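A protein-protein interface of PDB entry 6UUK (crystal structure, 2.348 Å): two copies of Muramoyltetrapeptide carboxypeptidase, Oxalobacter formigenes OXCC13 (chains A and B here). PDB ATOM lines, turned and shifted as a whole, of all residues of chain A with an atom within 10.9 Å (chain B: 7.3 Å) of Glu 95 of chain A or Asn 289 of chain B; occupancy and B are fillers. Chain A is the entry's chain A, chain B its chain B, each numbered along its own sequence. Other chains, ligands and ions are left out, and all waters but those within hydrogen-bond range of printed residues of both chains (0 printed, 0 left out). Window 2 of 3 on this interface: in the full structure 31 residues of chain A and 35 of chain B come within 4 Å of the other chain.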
ATOM      1  N   GLY A  62     -34.095 -27.389  -6.497  1.00  0.00           N
ATOM      2  CA  GLY A  62     -32.750 -26.851  -6.520  1.00  0.00           C
ATOM      3  C   GLY A  62     -31.725 -27.780  -5.907  1.00  0.00           C
ATOM      4  O   GLY A  62     -30.949 -27.373  -5.037  1.00  0.00           O
ATOM      5  N   GLY A  63     -31.709 -29.031  -6.355  1.00  0.00           N
ATOM      6  CA  GLY A  63     -30.777 -30.004  -5.823  1.00  0.00           C
ATOM      7  C   GLY A  63     -30.155 -30.891  -6.881  1.00  0.00           C
ATOM      8  O   GLY A  63     -30.850 -31.407  -7.761  1.00  0.00           O
ATOM      9  N   TYR A  64     -28.839 -31.070  -6.804  1.00  0.00           N
ATOM     10  CA  TYR A  64     -28.104 -31.950  -7.705  1.00  0.00           C
ATOM     11  C   TYR A  64     -27.946 -33.300  -7.013  1.00  0.00           C
ATOM     12  O   TYR A  64     -27.276 -33.400  -5.981  1.00  0.00           O
ATOM     13  CB  TYR A  64     -26.749 -31.346  -8.069  1.00  0.00           C
ATOM     14  CG  TYR A  64     -26.047 -32.032  -9.220  1.00  0.00           C
ATOM     15  CD1 TYR A  64     -26.292 -31.652 -10.532  1.00  0.00           C
ATOM     16  CD2 TYR A  64     -25.131 -33.051  -8.992  1.00  0.00           C
ATOM     17  CE1 TYR A  64     -25.650 -32.272 -11.588  1.00  0.00           C
ATOM     18  CE2 TYR A  64     -24.483 -33.677 -10.043  1.00  0.00           C
ATOM     19  CZ  TYR A  64     -24.747 -33.284 -11.338  1.00  0.00           C
ATOM     20  OH  TYR A  64     -24.106 -33.903 -12.386  1.00  0.00           O
ATOM     21  N   VAL A  65     -28.572 -34.329  -7.573  1.00  0.00           N
ATOM     22  CA  VAL A  65     -28.571 -35.659  -6.968  1.00  0.00           C
ATOM     23  C   VAL A  65     -27.847 -36.614  -7.911  1.00  0.00           C
ATOM     24  O   VAL A  65     -27.952 -36.459  -9.137  1.00  0.00           O
ATOM     25  CB  VAL A  65     -30.004 -36.129  -6.671  1.00  0.00           C
ATOM     26  CG1 VAL A  65     -30.002 -37.401  -5.838  1.00  0.00           C
ATOM     27  CG2 VAL A  65     -30.785 -35.031  -5.963  1.00  0.00           C
ATOM     28  N   PRO A  66     -27.078 -37.578  -7.399  1.00  0.00           N
ATOM     29  CA  PRO A  66     -26.458 -38.577  -8.278  1.00  0.00           C
ATOM     30  C   PRO A  66     -27.473 -39.218  -9.214  1.00  0.00           C
ATOM     31  O   PRO A  66     -28.628 -39.452  -8.850  1.00  0.00           O
ATOM     32  CB  PRO A  66     -25.872 -39.591  -7.293  1.00  0.00           C
ATOM     33  CG  PRO A  66     -25.522 -38.765  -6.104  1.00  0.00           C
ATOM     34  CD  PRO A  66     -26.567 -37.675  -6.019  1.00  0.00           C
ATOM     35  N   ASP A  67     -27.023 -39.504 -10.438  1.00  0.00           N
ATOM     36  CA  ASP A  67     -27.937 -39.930 -11.493  1.00  0.00           C
ATOM     37  C   ASP A  67     -28.497 -41.321 -11.226  1.00  0.00           C
ATOM     38  O   ASP A  67     -29.683 -41.575 -11.467  1.00  0.00           O
ATOM     39  CB  ASP A  67     -27.221 -39.890 -12.842  1.00  0.00           C
ATOM     40  CG  ASP A  67     -26.395 -38.631 -13.026  1.00  0.00           C
ATOM     41  OD1 ASP A  67     -26.829 -37.558 -12.556  1.00  0.00           O
ATOM     42  OD2 ASP A  67     -25.306 -38.715 -13.633  1.00  0.00           O
ATOM     43  N   ARG A  93     -29.009 -29.403 -15.879  1.00  0.00           N
ATOM     44  CA  ARG A  93     -28.170 -29.156 -14.713  1.00  0.00           C
ATOM     45  C   ARG A  93     -27.510 -27.786 -14.796  1.00  0.00           C
ATOM     46  O   ARG A  93     -27.193 -27.305 -15.885  1.00  0.00           O
ATOM     47  CB  ARG A  93     -27.105 -30.246 -14.576  1.00  0.00           C
ATOM     48  N   HIS A  94     -27.307 -27.156 -13.637  1.00  0.00           N
ATOM     49  CA  HIS A  94     -26.685 -25.833 -13.595  1.00  0.00           C
ATOM     50  C   HIS A  94     -26.060 -25.655 -12.210  1.00  0.00           C
ATOM     51  O   HIS A  94     -26.770 -25.353 -11.247  1.00  0.00           O
ATOM     52  CB  HIS A  94     -27.696 -24.739 -13.895  1.00  0.00           C
ATOM     53  CG  HIS A  94     -27.097 -23.370 -13.972  1.00  0.00           C
ATOM     54  ND1 HIS A  94     -26.053 -23.062 -14.817  1.00  0.00           N
ATOM     55  CD2 HIS A  94     -27.397 -22.226 -13.312  1.00  0.00           C
ATOM     56  CE1 HIS A  94     -25.734 -21.787 -14.674  1.00  0.00           C
ATOM     57  NE2 HIS A  94     -26.535 -21.258 -13.767  1.00  0.00           N
ATOM     58  N   GLU A  95     -24.745 -25.847 -12.131  1.00  0.00           N
ATOM     59  CA  GLU A  95     -23.960 -25.627 -10.909  1.00  0.00           C
ATOM     60  C   GLU A  95     -24.506 -26.555  -9.825  1.00  0.00           C
ATOM     61  O   GLU A  95     -24.616 -27.768 -10.065  1.00  0.00           O
ATOM     62  CB  GLU A  95     -23.971 -24.140 -10.573  1.00  0.00           C
ATOM     63  CG  GLU A  95     -23.457 -23.246 -11.689  1.00  0.00           C
ATOM     64  CD  GLU A  95     -23.636 -21.772 -11.382  1.00  0.00           C
ATOM     65  OE1 GLU A  95     -24.377 -21.449 -10.430  1.00  0.00           O
ATOM     66  OE2 GLU A  95     -23.035 -20.938 -12.090  1.00  0.00           O
ATOM     67  N   ARG A  96     -24.853 -26.049  -8.640  1.00  0.00           N
ATOM     68  CA  ARG A  96     -25.398 -26.881  -7.575  1.00  0.00           C
ATOM     69  C   ARG A  96     -26.831 -27.315  -7.837  1.00  0.00           C
ATOM     70  O   ARG A  96     -27.324 -28.214  -7.148  1.00  0.00           O
ATOM     71  CB  ARG A  96     -25.344 -26.130  -6.243  1.00  0.00           C
ATOM     72  CG  ARG A  96     -23.997 -25.522  -5.912  1.00  0.00           C
ATOM     73  CD  ARG A  96     -24.130 -24.507  -4.791  1.00  0.00           C
ATOM     74  NE  ARG A  96     -24.937 -25.018  -3.687  1.00  0.00           N
ATOM     75  CZ  ARG A  96     -24.442 -25.630  -2.618  1.00  0.00           C
ATOM     76  NH1 ARG A  96     -25.255 -26.062  -1.664  1.00  0.00           N
ATOM     77  NH2 ARG A  96     -23.133 -25.808  -2.499  1.00  0.00           N
ATOM     78  N   PHE A  97     -27.506 -26.704  -8.803  1.00  0.00           N
ATOM     79  CA  PHE A  97     -28.929 -26.907  -9.023  1.00  0.00           C
ATOM     80  C   PHE A  97     -29.167 -27.873 -10.178  1.00  0.00           C
ATOM     81  O   PHE A  97     -28.314 -28.064 -11.049  1.00  0.00           O
ATOM     82  CB  PHE A  97     -29.618 -25.568  -9.302  1.00  0.00           C
ATOM     83  CG  PHE A  97     -29.163 -24.455  -8.398  1.00  0.00           C
ATOM     84  CD1 PHE A  97     -29.769 -24.248  -7.171  1.00  0.00           C
ATOM     85  CD2 PHE A  97     -28.122 -23.620  -8.775  1.00  0.00           C
ATOM     86  CE1 PHE A  97     -29.349 -23.227  -6.337  1.00  0.00           C
ATOM     87  CE2 PHE A  97     -27.697 -22.599  -7.945  1.00  0.00           C
ATOM     88  CZ  PHE A  97     -28.312 -22.402  -6.726  1.00  0.00           C
ATOM     89  N   ALA A  98     -30.351 -28.486 -10.171  1.00  0.00           N
ATOM     90  CA  ALA A  98     -30.718 -29.437 -11.213  1.00  0.00           C
ATOM     91  C   ALA A  98     -31.008 -28.767 -12.548  1.00  0.00           C
ATOM     92  O   ALA A  98     -31.127 -29.471 -13.557  1.00  0.00           O
ATOM     93  CB  ALA A  98     -31.931 -30.257 -10.772  1.00  0.00           C
ATOM     94  N   ALA A  99     -31.124 -27.446 -12.577  1.00  0.00           N
ATOM     95  CA  ALA A  99     -31.373 -26.677 -13.794  1.00  0.00           C
ATOM     96  C   ALA A  99     -31.203 -25.203 -13.447  1.00  0.00           C
ATOM     97  O   ALA A  99     -30.773 -24.857 -12.339  1.00  0.00           O
ATOM     98  CB  ALA A  99     -32.759 -26.971 -14.370  1.00  0.00           C
ATOM     99  N   ASN A 100     -31.540 -24.330 -14.392  1.00  0.00           N
ATOM    100  CA  ASN A 100     -31.550 -22.902 -14.123  1.00  0.00           C
ATOM    101  C   ASN A 100     -32.789 -22.539 -13.309  1.00  0.00           C
ATOM    102  O   ASN A 100     -33.649 -23.378 -13.024  1.00  0.00           O
ATOM    103  CB  ASN A 100     -31.489 -22.112 -15.428  1.00  0.00           C
ATOM    104  CG  ASN A 100     -32.627 -22.449 -16.369  1.00  0.00           C
ATOM    105  OD1 ASN A 100     -33.727 -21.906 -16.252  1.00  0.00           O
ATOM    106  ND2 ASN A 100     -32.368 -23.347 -17.312  1.00  0.00           N
ATOM    107  N   ASP A 101     -32.887 -21.264 -12.924  1.00  0.00           N
ATOM    108  CA  ASP A 101     -34.023 -20.827 -12.120  1.00  0.00           C
ATOM    109  C   ASP A 101     -35.325 -20.913 -12.904  1.00  0.00           C
ATOM    110  O   ASP A 101     -36.354 -21.336 -12.365  1.00  0.00           O
ATOM    111  CB  ASP A 101     -33.794 -19.403 -11.613  1.00  0.00           C
ATOM    112  CG  ASP A 101     -32.630 -19.310 -10.647  1.00  0.00           C
ATOM    113  OD1 ASP A 101     -31.982 -20.347 -10.393  1.00  0.00           O
ATOM    114  OD2 ASP A 101     -32.362 -18.200 -10.141  1.00  0.00           O
ATOM    115  N   GLU A 102     -35.302 -20.524 -14.181  1.00  0.00           N
ATOM    116  CA  GLU A 102     -36.524 -20.546 -14.979  1.00  0.00           C
ATOM    117  C   GLU A 102     -36.957 -21.973 -15.290  1.00  0.00           C
ATOM    118  O   GLU A 102     -38.156 -22.277 -15.291  1.00  0.00           O
ATOM    119  CB  GLU A 102     -36.327 -19.750 -16.270  1.00  0.00           C
ATOM    120  CG  GLU A 102     -35.881 -18.312 -16.053  1.00  0.00           C
ATOM    121  CD  GLU A 102     -34.372 -18.173 -15.972  1.00  0.00           C
ATOM    122  OE1 GLU A 102     -33.785 -17.536 -16.870  1.00  0.00           O
ATOM    123  OE2 GLU A 102     -33.772 -18.708 -15.015  1.00  0.00           O
ATOM    124  N   ARG A 104     -36.132 -24.763 -13.453  1.00  0.00           N
ATOM    125  CA  ARG A 104     -36.588 -25.332 -12.190  1.00  0.00           C
ATOM    126  C   ARG A 104     -37.923 -24.736 -11.760  1.00  0.00           C
ATOM    127  O   ARG A 104     -38.677 -25.372 -11.015  1.00  0.00           O
ATOM    128  CB  ARG A 104     -35.528 -25.123 -11.108  1.00  0.00           C
ATOM    129  CG  ARG A 104     -34.482 -26.228 -11.055  1.00  0.00           C
ATOM    130  CD  ARG A 104     -33.192 -25.776 -10.384  1.00  0.00           C
ATOM    131  NE  ARG A 104     -33.425 -24.983  -9.180  1.00  0.00           N
ATOM    132  CZ  ARG A 104     -33.115 -23.695  -9.067  1.00  0.00           C
ATOM    133  NH1 ARG A 104     -33.360 -23.048  -7.935  1.00  0.00           N
ATOM    134  NH2 ARG A 104     -32.552 -23.056 -10.083  1.00  0.00           N
ATOM    135  N   ARG A 124     -34.368 -32.678  -3.697  1.00  0.00           N
ATOM    136  CA  ARG A 124     -33.362 -32.423  -2.678  1.00  0.00           C
ATOM    137  C   ARG A 124     -33.696 -31.121  -1.962  1.00  0.00           C
ATOM    138  O   ARG A 124     -34.310 -30.219  -2.537  1.00  0.00           O
ATOM    139  CB  ARG A 124     -31.954 -32.353  -3.289  1.00  0.00           C
ATOM    140  CG  ARG A 124     -30.822 -32.340  -2.274  1.00  0.00           C
ATOM    141  CD  ARG A 124     -29.474 -32.180  -2.957  1.00  0.00           C
ATOM    142  NE  ARG A 124     -28.373 -32.185  -1.999  1.00  0.00           N
ATOM    143  CZ  ARG A 124     -27.712 -33.276  -1.627  1.00  0.00           C
ATOM    144  NH1 ARG A 124     -28.039 -34.456  -2.135  1.00  0.00           N
ATOM    145  NH2 ARG A 124     -26.723 -33.187  -0.748  1.00  0.00           N
ATOM    146  N   TYR A 127     -30.484 -25.931  -1.352  1.00  0.00           N
ATOM    147  CA  TYR A 127     -30.684 -24.498  -1.512  1.00  0.00           C
ATOM    148  C   TYR A 127     -31.108 -24.223  -2.947  1.00  0.00           C
ATOM    149  O   TYR A 127     -30.560 -24.809  -3.882  1.00  0.00           O
ATOM    150  CB  TYR A 127     -29.411 -23.712  -1.173  1.00  0.00           C
ATOM    151  CG  TYR A 127     -29.477 -22.245  -1.539  1.00  0.00           C
ATOM    152  CD1 TYR A 127     -30.124 -21.332  -0.716  1.00  0.00           C
ATOM    153  CD2 TYR A 127     -28.891 -21.772  -2.707  1.00  0.00           C
ATOM    154  CE1 TYR A 127     -30.188 -19.992  -1.047  1.00  0.00           C
ATOM    155  CE2 TYR A 127     -28.950 -20.433  -3.046  1.00  0.00           C
ATOM    156  CZ  TYR A 127     -29.600 -19.548  -2.212  1.00  0.00           C
ATOM    157  OH  TYR A 127     -29.661 -18.214  -2.544  1.00  0.00           O
ATOM    158  N   GLY A 128     -32.081 -23.329  -3.111  1.00  0.00           N
ATOM    159  CA  GLY A 128     -32.501 -22.933  -4.440  1.00  0.00           C
ATOM    160  C   GLY A 128     -33.989 -22.704  -4.601  1.00  0.00           C
ATOM    161  O   GLY A 128     -34.432 -22.223  -5.648  1.00  0.00           O
ATOM    162  N   ARG A 131     -35.056 -18.907  -4.718  1.00  0.00           N
ATOM    163  CA  ARG A 131     -34.964 -18.352  -6.063  1.00  0.00           C
ATOM    164  C   ARG A 131     -36.256 -18.560  -6.840  1.00  0.00           C
ATOM    165  O   ARG A 131     -36.563 -17.785  -7.754  1.00  0.00           O
ATOM    166  CB  ARG A 131     -33.798 -18.990  -6.821  1.00  0.00           C
ATOM    167  CG  ARG A 131     -32.419 -18.689  -6.264  1.00  0.00           C
ATOM    168  CD  ARG A 131     -31.352 -19.283  -7.171  1.00  0.00           C
ATOM    169  NE  ARG A 131     -30.009 -18.807  -6.857  1.00  0.00           N
ATOM    170  CZ  ARG A 131     -28.941 -19.049  -7.610  1.00  0.00           C
ATOM    171  NH1 ARG A 131     -29.062 -19.759  -8.724  1.00  0.00           N
ATOM    172  NH2 ARG A 131     -27.753 -18.579  -7.255  1.00  0.00           N
ATOM    173  N   SER B 285     -16.585 -27.240  -2.967  1.00  0.00           N
ATOM    174  CA  SER B 285     -16.356 -28.631  -3.321  1.00  0.00           C
ATOM    175  C   SER B 285     -16.666 -28.833  -4.797  1.00  0.00           C
ATOM    176  O   SER B 285     -17.081 -27.907  -5.502  1.00  0.00           O
ATOM    177  CB  SER B 285     -17.201 -29.569  -2.450  1.00  0.00           C
ATOM    178  OG  SER B 285     -17.031 -30.916  -2.846  1.00  0.00           O
ATOM    179  N   ASP B 286     -16.459 -30.068  -5.267  1.00  0.00           N
ATOM    180  CA  ASP B 286     -16.788 -30.402  -6.648  1.00  0.00           C
ATOM    181  C   ASP B 286     -18.291 -30.387  -6.885  1.00  0.00           C
ATOM    182  O   ASP B 286     -18.733 -30.181  -8.021  1.00  0.00           O
ATOM    183  CB  ASP B 286     -16.215 -31.773  -7.011  1.00  0.00           C
ATOM    184  CG  ASP B 286     -16.688 -32.870  -6.077  1.00  0.00           C
ATOM    185  OD1 ASP B 286     -16.802 -32.607  -4.862  1.00  0.00           O
ATOM    186  OD2 ASP B 286     -16.946 -33.996  -6.556  1.00  0.00           O
ATOM    187  N   TYR B 287     -19.093 -30.609  -5.843  1.00  0.00           N
ATOM    188  CA  TYR B 287     -20.540 -30.584  -6.016  1.00  0.00           C
ATOM    189  C   TYR B 287     -21.075 -29.191  -6.317  1.00  0.00           C
ATOM    190  O   TYR B 287     -22.231 -29.069  -6.738  1.00  0.00           O
ATOM    191  CB  TYR B 287     -21.237 -31.151  -4.777  1.00  0.00           C
ATOM    192  CG  TYR B 287     -21.621 -32.608  -4.912  1.00  0.00           C
ATOM    193  CD1 TYR B 287     -21.216 -33.353  -6.012  1.00  0.00           C
ATOM    194  CD2 TYR B 287     -22.405 -33.233  -3.951  1.00  0.00           C
ATOM    195  CE1 TYR B 287     -21.569 -34.683  -6.144  1.00  0.00           C
ATOM    196  CE2 TYR B 287     -22.764 -34.562  -4.075  1.00  0.00           C
ATOM    197  CZ  TYR B 287     -22.343 -35.282  -5.173  1.00  0.00           C
ATOM    198  OH  TYR B 287     -22.697 -36.604  -5.301  1.00  0.00           O
ATOM    199  N   ASP B 288     -20.273 -28.144  -6.116  1.00  0.00           N
ATOM    200  CA  ASP B 288     -20.706 -26.808  -6.507  1.00  0.00           C
ATOM    201  C   ASP B 288     -20.775 -26.667  -8.022  1.00  0.00           C
ATOM    202  O   ASP B 288     -21.594 -25.893  -8.532  1.00  0.00           O
ATOM    203  CB  ASP B 288     -19.769 -25.756  -5.913  1.00  0.00           C
ATOM    204  CG  ASP B 288     -19.871 -25.672  -4.404  1.00  0.00           C
ATOM    205  OD1 ASP B 288     -21.001 -25.750  -3.878  1.00  0.00           O
ATOM    206  OD2 ASP B 288     -18.822 -25.532  -3.743  1.00  0.00           O
ATOM    207  N   ASN B 289     -19.934 -27.407  -8.746  1.00  0.00           N
ATOM    208  CA  ASN B 289     -19.943 -27.436 -10.209  1.00  0.00           C
ATOM    209  C   ASN B 289     -19.802 -26.030 -10.789  1.00  0.00           C
ATOM    210  O   ASN B 289     -20.595 -25.587 -11.622  1.00  0.00           O
ATOM    211  CB  ASN B 289     -21.204 -28.128 -10.733  1.00  0.00           C
ATOM    212  CG  ASN B 289     -21.104 -28.490 -12.202  1.00  0.00           C
ATOM    213  OD1 ASN B 289     -20.008 -28.659 -12.737  1.00  0.00           O
ATOM    214  ND2 ASN B 289     -22.249 -28.608 -12.864  1.00  0.00           N
ATOM    215  N   GLY B 290     -18.774 -25.321 -10.331  1.00  0.00           N
ATOM    216  CA  GLY B 290     -18.514 -23.974 -10.786  1.00  0.00           C
ATOM    217  C   GLY B 290     -19.153 -22.878  -9.964  1.00  0.00           C
ATOM    218  O   GLY B 290     -18.903 -21.697 -10.238  1.00  0.00           O
ATOM    219  N   TYR B 291     -19.970 -23.221  -8.971  1.00  0.00           N
ATOM    220  CA  TYR B 291     -20.593 -22.214  -8.125  1.00  0.00           C
ATOM    221  C   TYR B 291     -19.593 -21.716  -7.091  1.00  0.00           C
ATOM    222  O   TYR B 291     -18.934 -22.513  -6.416  1.00  0.00           O
ATOM    223  CB  TYR B 291     -21.833 -22.781  -7.433  1.00  0.00           C
ATOM    224  CG  TYR B 291     -22.646 -21.739  -6.696  1.00  0.00           C
ATOM    225  CD1 TYR B 291     -22.408 -21.462  -5.356  1.00  0.00           C
ATOM    226  CD2 TYR B 291     -23.648 -21.029  -7.344  1.00  0.00           C
ATOM    227  CE1 TYR B 291     -23.148 -20.508  -4.681  1.00  0.00           C
ATOM    228  CE2 TYR B 291     -24.393 -20.074  -6.677  1.00  0.00           C
ATOM    229  CZ  TYR B 291     -24.138 -19.818  -5.346  1.00  0.00           C
ATOM    230  OH  TYR B 291     -24.877 -18.869  -4.679  1.00  0.00           O
ATOM    231  N   ASP B 292     -19.486 -20.398  -6.967  1.00  0.00           N
ATOM    232  CA  ASP B 292     -18.553 -19.784  -6.033  1.00  0.00           C
ATOM    233  C   ASP B 292     -19.049 -18.372  -5.728  1.00  0.00           C
ATOM    234  O   ASP B 292     -20.245 -18.083  -5.858  1.00  0.00           O
ATOM    235  CB  ASP B 292     -17.128 -19.806  -6.609  1.00  0.00           C
ATOM    236  CG  ASP B 292     -17.069 -19.308  -8.040  1.00  0.00           C
ATOM    237  OD1 ASP B 292     -18.114 -18.865  -8.562  1.00  0.00           O
ATOM    238  OD2 ASP B 292     -15.979 -19.363  -8.645  1.00  0.00           O
ATOM    239  N   ASN B 294     -18.068 -15.600  -7.367  1.00  0.00           N
ATOM    240  CA  ASN B 294     -18.295 -14.875  -8.612  1.00  0.00           C
ATOM    241  C   ASN B 294     -19.641 -15.238  -9.227  1.00  0.00           C
ATOM    242  O   ASN B 294     -20.366 -14.361  -9.709  1.00  0.00           O
ATOM    243  CB  ASN B 294     -17.164 -15.155  -9.600  1.00  0.00           C
ATOM    244  CG  ASN B 294     -15.837 -14.580  -9.148  1.00  0.00           C
ATOM    245  OD1 ASN B 294     -15.786 -13.537  -8.497  1.00  0.00           O
ATOM    246  ND2 ASN B 294     -14.750 -15.260  -9.495  1.00  0.00           N
ATOM    247  N   ALA B 295     -19.990 -16.528  -9.221  1.00  0.00           N
ATOM    248  CA  ALA B 295     -21.281 -16.945  -9.759  1.00  0.00           C
ATOM    249  C   ALA B 295     -22.433 -16.433  -8.906  1.00  0.00           C
ATOM    250  O   ALA B 295     -23.531 -16.198  -9.425  1.00  0.00           O
ATOM    251  CB  ALA B 295     -21.339 -18.467  -9.872  1.00  0.00           C
ATOM    252  N   MET B 296     -22.208 -16.255  -7.608  1.00  0.00           N
ATOM    253  CA  MET B 296     -23.226 -15.715  -6.717  1.00  0.00           C
ATOM    254  C   MET B 296     -23.350 -14.208  -6.909  1.00  0.00           C
ATOM    255  O   MET B 296     -24.453 -13.660  -6.910  1.00  0.00           O
ATOM    256  CB  MET B 296     -22.892 -16.045  -5.261  1.00  0.00           C
ATOM    257  CG  MET B 296     -23.931 -15.578  -4.255  1.00  0.00           C
ATOM    258  SD  MET B 296     -23.661 -13.755  -3.611  1.00  0.00           S
ATOM    259  CE  MET B 296     -21.997 -14.026  -2.633  1.00  0.00           C
ATOM    260  N   TRP B 299     -25.206 -13.502 -10.138  1.00  0.00           N
ATOM    261  CA  TRP B 299     -26.637 -13.719  -9.955  1.00  0.00           C
ATOM    262  C   TRP B 299     -27.247 -12.660  -9.047  1.00  0.00           C
ATOM    263  O   TRP B 299     -28.414 -12.293  -9.222  1.00  0.00           O
ATOM    264  CB  TRP B 299     -26.891 -15.116  -9.389  1.00  0.00           C
ATOM    265  CG  TRP B 299     -28.340 -15.497  -9.358  1.00  0.00           C
ATOM    266  CD1 TRP B 299     -29.027 -16.182 -10.317  1.00  0.00           C
ATOM    267  CD2 TRP B 299     -29.283 -15.215  -8.315  1.00  0.00           C
ATOM    268  NE1 TRP B 299     -30.338 -16.343  -9.937  1.00  0.00           N
ATOM    269  CE2 TRP B 299     -30.520 -15.758  -8.713  1.00  0.00           C
ATOM    270  CE3 TRP B 299     -29.200 -14.553  -7.086  1.00  0.00           C
ATOM    271  CZ2 TRP B 299     -31.665 -15.662  -7.924  1.00  0.00           C
ATOM    272  CZ3 TRP B 299     -30.337 -14.459  -6.305  1.00  0.00           C
ATOM    273  CH2 TRP B 299     -31.553 -15.011  -6.727  1.00  0.00           C
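Of the 12 printed residues of chain B, 6 touch a printed residue of chain A.
Hydrophobic or aromatic side chains of chain B within 4 Å of the printed part of chain A: Tyr 287, Tyr 291, Ala 295 and Trp 299.
Among the printed residues, Asp or Glu carboxylates within 4 Å of a Lys or Arg side-chain nitrogen of the other chain: Arg 96 of chain A with Asp 288 of chain B.
NH2 of Arg 96 of chain A lies within salt-bridge range of OD1 of Asp 288 of chain B.
The side-chain carboxylate (OD2) of Asp 101 of chain A is in hydrogen-bond range of the indole nitrogen (NE1) of Trp 299 of chain B (2.8 Å).
The backbone NH (N) of Tyr 64 of chain A sits at hydrogen-bond distance from the backbone carbonyl oxygen (O) of Arg 96 of chain A, 3.3 Å away.
OD1 of Asp 101 of chain A lies within salt-bridge range of NH2 of Arg 104 of chain A (2.8 Å).
OD1 of Asp 101 of chain A lies within salt-bridge range of NH1 of Arg 131 of chain A, at 3.4 Å.
The backbone NH (N) of Ser 285 of chain B lies within hydrogen-bond range of the side-chain carboxylate (OD2) of Asp 288 of chain B (2.9 Å).
The side-chain carboxylate (OD1) of Asp 292 of chain B is in hydrogen-bond range of the backbone NH (N) of Ala 295 of chain B.
No position is printed for both chains.
Printed residues of chain B within 4 Å of Pro 66 of chain A: Tyr 287.
Of the printed residues of chain B, Glu 95 of chain A touches Asp 288, Asn 289, Tyr 291 and Ala 295.
Of the printed residues of chain B, Arg 96 of chain A touches Tyr 287, Asp 288 and Tyr 291.
Printed residues of chain B within 4 Å of Asp 101 of chain A: Trp 299 (2.8 Å).
Printed residues of chain B within 4 Å of Arg 131 of chain A: Tyr 291 (3.7 Å) and Trp 299 (3.5 Å).
Ser 285 of chain B touches none of the printed residues of chain A.
Printed residues of chain A within 4 Å of Asp 288 of chain B: Glu 95 and Arg 96.
Of chain A, only Glu 95 (3.4 Å) comes within 4 Å of Asn 289 of chain B.
No residue of chain A comes within 4 Å of Gly 290 of chain B.
Tyr 291 of chain B touches three residues of chain A.
Asn 294 of chain B touches none of the printed residues of chain A.
Ala 295 of chain B touches just one residue of chain A: Glu 95 (3.7 Å).
Printed residues of chain A within 4 Å of Trp 299 of chain B: Asp 101 and Arg 131.
Tyr 287 of chain B touches Pro 66 of chain A (OH to CG, 3.6 Å).
Glu 95 of chain A touches Asp 288 of chain B (C to O, 3.3 Å).
CA of Glu 95 of chain A touches O of Asn 289 of chain B, 3.4 Å away.
Glu 95 of chain A touches Tyr 291 of chain B.
CB of Ala 295 of chain B touches OE2 of Glu 95 of chain A, 3.7 Å away.
Tyr 287 of chain B touches Arg 96 of chain A.
Arg 96 of chain A touches Tyr 291 of chain B (CD to CD1, 3.5 Å).
CE2 of Tyr 291 of chain B touches NH2 of Arg 131 of chain A, at 3.7 Å.
CG of Arg 131 of chain A touches CZ2 of Trp 299 of chain B (3.5 Å).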
